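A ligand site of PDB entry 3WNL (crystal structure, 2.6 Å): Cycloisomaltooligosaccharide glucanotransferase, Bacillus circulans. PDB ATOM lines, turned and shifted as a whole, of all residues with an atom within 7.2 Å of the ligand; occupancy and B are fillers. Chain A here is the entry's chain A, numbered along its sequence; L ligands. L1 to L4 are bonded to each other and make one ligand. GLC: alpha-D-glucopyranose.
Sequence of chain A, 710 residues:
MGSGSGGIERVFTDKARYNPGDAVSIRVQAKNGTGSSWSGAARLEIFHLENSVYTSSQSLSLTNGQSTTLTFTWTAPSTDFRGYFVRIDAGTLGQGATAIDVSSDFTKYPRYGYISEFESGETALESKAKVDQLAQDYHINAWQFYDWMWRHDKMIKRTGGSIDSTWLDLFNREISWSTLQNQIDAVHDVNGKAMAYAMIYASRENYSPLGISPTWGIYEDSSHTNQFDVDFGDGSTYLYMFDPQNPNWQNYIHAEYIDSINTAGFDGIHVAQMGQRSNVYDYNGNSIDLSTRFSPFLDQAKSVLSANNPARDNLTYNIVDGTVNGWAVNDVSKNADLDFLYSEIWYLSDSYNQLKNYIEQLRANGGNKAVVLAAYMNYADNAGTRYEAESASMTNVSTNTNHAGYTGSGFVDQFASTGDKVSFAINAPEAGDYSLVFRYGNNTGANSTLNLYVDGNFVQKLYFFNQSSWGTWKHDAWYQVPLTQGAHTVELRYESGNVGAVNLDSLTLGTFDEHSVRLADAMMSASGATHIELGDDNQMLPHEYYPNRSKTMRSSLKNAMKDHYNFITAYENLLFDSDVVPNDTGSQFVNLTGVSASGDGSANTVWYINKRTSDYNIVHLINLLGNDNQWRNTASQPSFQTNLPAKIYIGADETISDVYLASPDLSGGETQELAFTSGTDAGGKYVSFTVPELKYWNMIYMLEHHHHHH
The backbone NH (N) of Gln 414 lies within hydrogen-bond range of an oxygen (O4) of GLC L2 (3.0 Å). An oxygen (O2) of GLC L3 is in hydrogen-bond range of the side-chain amide oxygen of Gln 414. OD1 of Asn 503 is in hydrogen-bond range of O4 of GLC L2 (2.6 Å). NE2 of His 403 lies within hydrogen-bond range of O2 of GLC L2.
The backbone NH of Gly 441 lies within hydrogen-bond range of the backbone carbonyl oxygen of Asn 503. OG1 of Thr 444 is in hydrogen-bond range of O of Ala 446, at 3.0 Å. The backbone carbonyl oxygen (O) of Ala 501 lies within hydrogen-bond range of the side-chain hydroxyl (OG) of Ser 448 (2.6 Å).
Residues that only touch the ligand: Thr 444 (3.9 Å), Trp 470 (3.3 Å) and Ala 501 (3.9 Å). Hydrophobic or aromatic side chains that line the ligand: His 403, Trp 470 and Ala 501. Within 4 Å of the ligand: His 403, Gln 414, Thr 444, Trp 470, Ala 501 and Asn 503. The nearest printed residue that does not touch the ligand is Ala 416 (4.002 Å).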
ATOM      1  N   ASN A 400     -21.773 -11.007  16.608  1.00  0.00           N
ATOM      2  CA  ASN A 400     -22.753 -11.233  15.595  1.00  0.00           C
ATOM      3  C   ASN A 400     -23.690 -10.053  15.531  1.00  0.00           C
ATOM      4  O   ASN A 400     -23.589  -9.153  16.372  1.00  0.00           O
ATOM      5  CB  ASN A 400     -23.516 -12.516  15.884  1.00  0.00           C
ATOM      6  CG  ASN A 400     -23.933 -13.189  14.624  1.00  0.00           C
ATOM      7  OD1 ASN A 400     -24.374 -12.539  13.698  1.00  0.00           O
ATOM      8  ND2 ASN A 400     -23.745 -14.465  14.559  1.00  0.00           N
ATOM      9  N   ASN A 402     -27.143 -10.774  13.895  1.00  0.00           N
ATOM     10  CA  ASN A 402     -28.253 -11.413  13.180  1.00  0.00           C
ATOM     11  C   ASN A 402     -29.589 -11.557  13.987  1.00  0.00           C
ATOM     12  O   ASN A 402     -30.252 -12.571  13.924  1.00  0.00           O
ATOM     13  CB  ASN A 402     -27.752 -12.773  12.644  1.00  0.00           C
ATOM     14  CG  ASN A 402     -27.407 -13.761  13.761  1.00  0.00           C
ATOM     15  OD1 ASN A 402     -27.028 -13.374  14.883  1.00  0.00           O
ATOM     16  ND2 ASN A 402     -27.551 -15.047  13.462  1.00  0.00           N
ATOM     17  N   HIS A 403     -29.936 -10.513  14.733  1.00  0.00           N
ATOM     18  CA  HIS A 403     -31.195 -10.384  15.518  1.00  0.00           C
ATOM     19  C   HIS A 403     -31.272  -8.907  15.922  1.00  0.00           C
ATOM     20  O   HIS A 403     -30.268  -8.308  16.372  1.00  0.00           O
ATOM     21  CB  HIS A 403     -31.209 -11.230  16.804  1.00  0.00           C
ATOM     22  CG  HIS A 403     -31.240 -12.704  16.576  1.00  0.00           C
ATOM     23  ND1 HIS A 403     -32.313 -13.360  16.013  1.00  0.00           N
ATOM     24  CD2 HIS A 403     -30.320 -13.667  16.874  1.00  0.00           C
ATOM     25  CE1 HIS A 403     -32.052 -14.657  15.959  1.00  0.00           C
ATOM     26  NE2 HIS A 403     -30.854 -14.870  16.462  1.00  0.00           N
ATOM     27  N   PHE A 411     -23.551  -7.904  19.168  1.00  0.00           N
ATOM     28  CA  PHE A 411     -23.582  -8.600  20.415  1.00  0.00           C
ATOM     29  C   PHE A 411     -22.795  -9.898  20.342  1.00  0.00           C
ATOM     30  O   PHE A 411     -22.324 -10.317  19.281  1.00  0.00           O
ATOM     31  CB  PHE A 411     -25.032  -8.894  20.775  1.00  0.00           C
ATOM     32  CG  PHE A 411     -25.757  -9.671  19.732  1.00  0.00           C
ATOM     33  CD1 PHE A 411     -26.403  -9.036  18.708  1.00  0.00           C
ATOM     34  CD2 PHE A 411     -25.783 -11.046  19.797  1.00  0.00           C
ATOM     35  CE1 PHE A 411     -27.085  -9.777  17.738  1.00  0.00           C
ATOM     36  CE2 PHE A 411     -26.454 -11.797  18.847  1.00  0.00           C
ATOM     37  CZ  PHE A 411     -27.102 -11.152  17.813  1.00  0.00           C
ATOM     38  N   VAL A 412     -22.668 -10.542  21.496  1.00  0.00           N
ATOM     39  CA  VAL A 412     -21.955 -11.781  21.561  1.00  0.00           C
ATOM     40  C   VAL A 412     -22.993 -12.895  21.612  1.00  0.00           C
ATOM     41  O   VAL A 412     -23.878 -12.870  22.459  1.00  0.00           O
ATOM     42  CB  VAL A 412     -20.993 -11.793  22.779  1.00  0.00           C
ATOM     43  CG1 VAL A 412     -20.389 -13.169  22.977  1.00  0.00           C
ATOM     44  CG2 VAL A 412     -19.904 -10.721  22.610  1.00  0.00           C
ATOM     45  N   ASP A 413     -22.874 -13.826  20.669  1.00  0.00           N
ATOM     46  CA  ASP A 413     -23.785 -14.931  20.534  1.00  0.00           C
ATOM     47  C   ASP A 413     -23.205 -16.175  21.154  1.00  0.00           C
ATOM     48  O   ASP A 413     -22.172 -16.099  21.816  1.00  0.00           O
ATOM     49  CB  ASP A 413     -24.096 -15.184  19.046  1.00  0.00           C
ATOM     50  CG  ASP A 413     -22.862 -15.567  18.226  1.00  0.00           C
ATOM     51  OD1 ASP A 413     -21.759 -15.774  18.795  1.00  0.00           O
ATOM     52  OD2 ASP A 413     -22.995 -15.639  16.998  1.00  0.00           O
ATOM     53  N   GLN A 414     -23.909 -17.303  20.967  1.00  0.00           N
ATOM     54  CA  GLN A 414     -23.347 -18.643  21.105  1.00  0.00           C
ATOM     55  C   GLN A 414     -22.514 -18.763  22.345  1.00  0.00           C
ATOM     56  O   GLN A 414     -21.365 -19.208  22.321  1.00  0.00           O
ATOM     57  CB  GLN A 414     -22.476 -18.988  19.891  1.00  0.00           C
ATOM     58  CG  GLN A 414     -23.243 -19.202  18.586  1.00  0.00           C
ATOM     59  CD  GLN A 414     -24.194 -20.376  18.669  1.00  0.00           C
ATOM     60  OE1 GLN A 414     -24.103 -21.213  19.588  1.00  0.00           O
ATOM     61  NE2 GLN A 414     -25.116 -20.443  17.722  1.00  0.00           N
ATOM     62  N   PHE A 415     -23.093 -18.297  23.433  1.00  0.00           N
ATOM     63  CA  PHE A 415     -22.412 -18.255  24.680  1.00  0.00           C
ATOM     64  C   PHE A 415     -23.042 -19.396  25.457  1.00  0.00           C
ATOM     65  O   PHE A 415     -23.825 -19.177  26.392  1.00  0.00           O
ATOM     66  CB  PHE A 415     -22.645 -16.892  25.317  1.00  0.00           C
ATOM     67  CG  PHE A 415     -21.793 -16.595  26.506  1.00  0.00           C
ATOM     68  CD1 PHE A 415     -20.995 -17.568  27.099  1.00  0.00           C
ATOM     69  CD2 PHE A 415     -21.847 -15.349  27.086  1.00  0.00           C
ATOM     70  CE1 PHE A 415     -20.241 -17.272  28.214  1.00  0.00           C
ATOM     71  CE2 PHE A 415     -21.104 -15.045  28.211  1.00  0.00           C
ATOM     72  CZ  PHE A 415     -20.295 -16.016  28.775  1.00  0.00           C
ATOM     73  N   ALA A 416     -22.677 -20.604  25.039  1.00  0.00           N
ATOM     74  CA  ALA A 416     -23.433 -21.806  25.368  1.00  0.00           C
ATOM     75  C   ALA A 416     -22.633 -23.010  25.908  1.00  0.00           C
ATOM     76  O   ALA A 416     -23.198 -24.113  25.956  1.00  0.00           O
ATOM     77  CB  ALA A 416     -24.173 -22.239  24.111  1.00  0.00           C
ATOM     78  N   SER A 417     -21.356 -22.848  26.270  1.00  0.00           N
ATOM     79  CA  SER A 417     -20.541 -24.038  26.650  1.00  0.00           C
ATOM     80  C   SER A 417     -19.335 -23.720  27.502  1.00  0.00           C
ATOM     81  O   SER A 417     -18.835 -22.596  27.502  1.00  0.00           O
ATOM     82  CB  SER A 417     -20.119 -24.885  25.420  1.00  0.00           C
ATOM     83  OG  SER A 417     -20.405 -24.240  24.189  1.00  0.00           O
ATOM     84  N   GLY A 441     -30.238 -11.943  25.516  1.00  0.00           N
ATOM     85  CA  GLY A 441     -31.285 -12.686  24.852  1.00  0.00           C
ATOM     86  C   GLY A 441     -31.228 -14.126  25.299  1.00  0.00           C
ATOM     87  O   GLY A 441     -30.164 -14.675  25.450  1.00  0.00           O
ATOM     88  N   ASN A 443     -33.590 -17.740  24.423  1.00  0.00           N
ATOM     89  CA  ASN A 443     -34.740 -18.407  23.807  1.00  0.00           C
ATOM     90  C   ASN A 443     -34.362 -19.868  23.655  1.00  0.00           C
ATOM     91  O   ASN A 443     -34.287 -20.419  22.557  1.00  0.00           O
ATOM     92  CB  ASN A 443     -35.140 -17.775  22.451  1.00  0.00           C
ATOM     93  CG  ASN A 443     -36.422 -18.368  21.861  1.00  0.00           C
ATOM     94  OD1 ASN A 443     -36.598 -18.416  20.633  1.00  0.00           O
ATOM     95  ND2 ASN A 443     -37.313 -18.849  22.729  1.00  0.00           N
ATOM     96  N   THR A 444     -34.060 -20.459  24.797  1.00  0.00           N
ATOM     97  CA  THR A 444     -33.622 -21.835  24.869  1.00  0.00           C
ATOM     98  C   THR A 444     -34.746 -22.674  25.401  1.00  0.00           C
ATOM     99  O   THR A 444     -34.649 -23.892  25.413  1.00  0.00           O
ATOM    100  CB  THR A 444     -32.418 -22.003  25.832  1.00  0.00           C
ATOM    101  OG1 THR A 444     -32.724 -21.455  27.142  1.00  0.00           O
ATOM    102  CG2 THR A 444     -31.164 -21.358  25.211  1.00  0.00           C
ATOM    103  N   GLY A 445     -35.799 -22.010  25.863  1.00  0.00           N
ATOM    104  CA  GLY A 445     -36.907 -22.687  26.489  1.00  0.00           C
ATOM    105  C   GLY A 445     -36.790 -22.742  27.994  1.00  0.00           C
ATOM    106  O   GLY A 445     -37.780 -23.091  28.661  1.00  0.00           O
ATOM    107  N   ALA A 446     -35.611 -22.434  28.555  1.00  0.00           N
ATOM    108  CA  ALA A 446     -35.558 -22.214  30.023  1.00  0.00           C
ATOM    109  C   ALA A 446     -34.582 -21.166  30.489  1.00  0.00           C
ATOM    110  O   ALA A 446     -33.877 -20.519  29.707  1.00  0.00           O
ATOM    111  CB  ALA A 446     -35.300 -23.512  30.810  1.00  0.00           C
ATOM    112  N   SER A 448     -31.252 -19.732  31.883  1.00  0.00           N
ATOM    113  CA  SER A 448     -29.859 -19.918  31.463  1.00  0.00           C
ATOM    114  C   SER A 448     -28.974 -19.303  32.568  1.00  0.00           C
ATOM    115  O   SER A 448     -29.382 -18.316  33.241  1.00  0.00           O
ATOM    116  CB  SER A 448     -29.611 -19.233  30.133  1.00  0.00           C
ATOM    117  OG  SER A 448     -30.052 -20.002  29.031  1.00  0.00           O
ATOM    118  N   TRP A 470     -35.508 -14.912  20.367  1.00  0.00           N
ATOM    119  CA  TRP A 470     -34.150 -14.371  20.248  1.00  0.00           C
ATOM    120  C   TRP A 470     -34.177 -12.915  19.743  1.00  0.00           C
ATOM    121  O   TRP A 470     -33.167 -12.229  19.764  1.00  0.00           O
ATOM    122  CB  TRP A 470     -33.312 -15.237  19.284  1.00  0.00           C
ATOM    123  CG  TRP A 470     -32.927 -16.645  19.754  1.00  0.00           C
ATOM    124  CD1 TRP A 470     -33.254 -17.820  19.140  1.00  0.00           C
ATOM    125  CD2 TRP A 470     -32.108 -17.008  20.889  1.00  0.00           C
ATOM    126  NE1 TRP A 470     -32.710 -18.887  19.822  1.00  0.00           N
ATOM    127  CE2 TRP A 470     -32.015 -18.428  20.898  1.00  0.00           C
ATOM    128  CE3 TRP A 470     -31.456 -16.280  21.898  1.00  0.00           C
ATOM    129  CZ2 TRP A 470     -31.309 -19.125  21.883  1.00  0.00           C
ATOM    130  CZ3 TRP A 470     -30.750 -16.977  22.874  1.00  0.00           C
ATOM    131  CH2 TRP A 470     -30.687 -18.391  22.861  1.00  0.00           C
ATOM    132  N   GLY A 500     -27.820 -23.714  29.661  1.00  0.00           N
ATOM    133  CA  GLY A 500     -28.502 -22.962  28.647  1.00  0.00           C
ATOM    134  C   GLY A 500     -27.589 -22.236  27.704  1.00  0.00           C
ATOM    135  O   GLY A 500     -26.684 -22.817  27.148  1.00  0.00           O
ATOM    136  N   ALA A 501     -27.837 -20.965  27.517  1.00  0.00           N
ATOM    137  CA  ALA A 501     -27.081 -20.199  26.579  1.00  0.00           C
ATOM    138  C   ALA A 501     -27.685 -18.826  26.621  1.00  0.00           C
ATOM    139  O   ALA A 501     -28.747 -18.679  27.213  1.00  0.00           O
ATOM    140  CB  ALA A 501     -27.178 -20.809  25.193  1.00  0.00           C
ATOM    141  N   VAL A 502     -26.985 -17.820  26.065  1.00  0.00           N
ATOM    142  CA  VAL A 502     -27.474 -16.430  25.961  1.00  0.00           C
ATOM    143  C   VAL A 502     -26.767 -15.687  24.820  1.00  0.00           C
ATOM    144  O   VAL A 502     -25.688 -16.086  24.374  1.00  0.00           O
ATOM    145  CB  VAL A 502     -27.264 -15.572  27.256  1.00  0.00           C
ATOM    146  CG1 VAL A 502     -27.589 -16.347  28.541  1.00  0.00           C
ATOM    147  CG2 VAL A 502     -25.856 -15.016  27.330  1.00  0.00           C
ATOM    148  N   ASN A 503     -27.387 -14.632  24.295  1.00  0.00           N
ATOM    149  CA  ASN A 503     -26.642 -13.618  23.571  1.00  0.00           C
ATOM    150  C   ASN A 503     -26.458 -12.467  24.570  1.00  0.00           C
ATOM    151  O   ASN A 503     -27.370 -12.132  25.322  1.00  0.00           O
ATOM    152  CB  ASN A 503     -27.377 -13.152  22.300  1.00  0.00           C
ATOM    153  CG  ASN A 503     -27.724 -14.304  21.336  1.00  0.00           C
ATOM    154  OD1 ASN A 503     -27.006 -15.299  21.255  1.00  0.00           O
ATOM    155  ND2 ASN A 503     -28.853 -14.170  20.624  1.00  0.00           N
HETATM  156  C1  GLC L   1     -27.914 -21.477  13.373  1.00  0.00           C
HETATM  157  C2  GLC L   1     -26.707 -21.936  14.191  1.00  0.00           C
HETATM  158  C3  GLC L   1     -27.061 -23.242  14.905  1.00  0.00           C
HETATM  159  C4  GLC L   1     -28.301 -23.072  15.811  1.00  0.00           C
HETATM  160  C5  GLC L   1     -29.388 -22.137  15.246  1.00  0.00           C
HETATM  161  C6  GLC L   1     -30.096 -21.387  16.374  1.00  0.00           C
HETATM  162  O1  GLC L   1     -28.281 -22.481  12.440  1.00  0.00           O
HETATM  163  O2  GLC L   1     -25.565 -22.079  13.351  1.00  0.00           O
HETATM  164  O3  GLC L   1     -25.936 -23.669  15.641  1.00  0.00           O
HETATM  165  O4  GLC L   1     -28.904 -24.333  16.046  1.00  0.00           O
HETATM  166  O5  GLC L   1     -28.978 -21.183  14.268  1.00  0.00           O
HETATM  167  O6  GLC L   1     -29.212 -20.473  17.034  1.00  0.00           O
HETATM  168  C1  GLC L   2     -29.865 -19.745  18.113  1.00  0.00           C
HETATM  169  C2  GLC L   2     -29.715 -18.211  17.987  1.00  0.00           C
HETATM  170  C3  GLC L   2     -28.386 -17.652  18.508  1.00  0.00           C
HETATM  171  C4  GLC L   2     -28.089 -18.206  19.910  1.00  0.00           C
HETATM  172  C5  GLC L   2     -28.130 -19.723  19.812  1.00  0.00           C
HETATM  173  C6  GLC L   2     -27.727 -20.433  21.095  1.00  0.00           C
HETATM  174  O2  GLC L   2     -29.971 -17.774  16.664  1.00  0.00           O
HETATM  175  O3  GLC L   2     -28.419 -16.234  18.512  1.00  0.00           O
HETATM  176  O4  GLC L   2     -26.840 -17.798  20.406  1.00  0.00           O
HETATM  177  O5  GLC L   2     -29.429 -20.159  19.404  1.00  0.00           O
HETATM  178  O6  GLC L   2     -27.628 -21.767  20.675  1.00  0.00           O
HETATM  179  C1  GLC L   3     -27.379 -22.696  21.759  1.00  0.00           C
HETATM  180  C2  GLC L   3     -26.487 -23.793  21.172  1.00  0.00           C
HETATM  181  C3  GLC L   3     -27.244 -24.746  20.236  1.00  0.00           C
HETATM  182  C4  GLC L   3     -28.567 -25.169  20.868  1.00  0.00           C
HETATM  183  C5  GLC L   3     -29.333 -23.913  21.312  1.00  0.00           C
HETATM  184  C6  GLC L   3     -30.730 -24.203  21.854  1.00  0.00           C
HETATM  185  O2  GLC L   3     -25.477 -23.177  20.421  1.00  0.00           O
HETATM  186  O3  GLC L   3     -26.476 -25.893  19.914  1.00  0.00           O
HETATM  187  O4  GLC L   3     -29.271 -25.985  19.946  1.00  0.00           O
HETATM  188  O5  GLC L   3     -28.561 -23.251  22.304  1.00  0.00           O
HETATM  189  O6  GLC L   3     -30.828 -25.600  22.025  1.00  0.00           O
HETATM  190  C1  GLC L   4     -32.044 -25.998  22.672  1.00  0.00           C
HETATM  191  C2  GLC L   4     -31.673 -26.352  24.101  1.00  0.00           C
HETATM  192  C3  GLC L   4     -30.957 -27.702  24.194  1.00  0.00           C
HETATM  193  C4  GLC L   4     -31.485 -28.777  23.234  1.00  0.00           C
HETATM  194  C5  GLC L   4     -31.892 -28.237  21.857  1.00  0.00           C
HETATM  195  C6  GLC L   4     -32.672 -29.297  21.078  1.00  0.00           C
HETATM  196  O2  GLC L   4     -30.814 -25.349  24.602  1.00  0.00           O
HETATM  197  O3  GLC L   4     -31.088 -28.190  25.522  1.00  0.00           O
HETATM  198  O4  GLC L   4     -30.440 -29.687  23.017  1.00  0.00           O
HETATM  199  O5  GLC L   4     -32.685 -27.082  22.018  1.00  0.00           O
HETATM  200  O6  GLC L   4     -33.956 -29.461  21.656  1.00  0.00           O
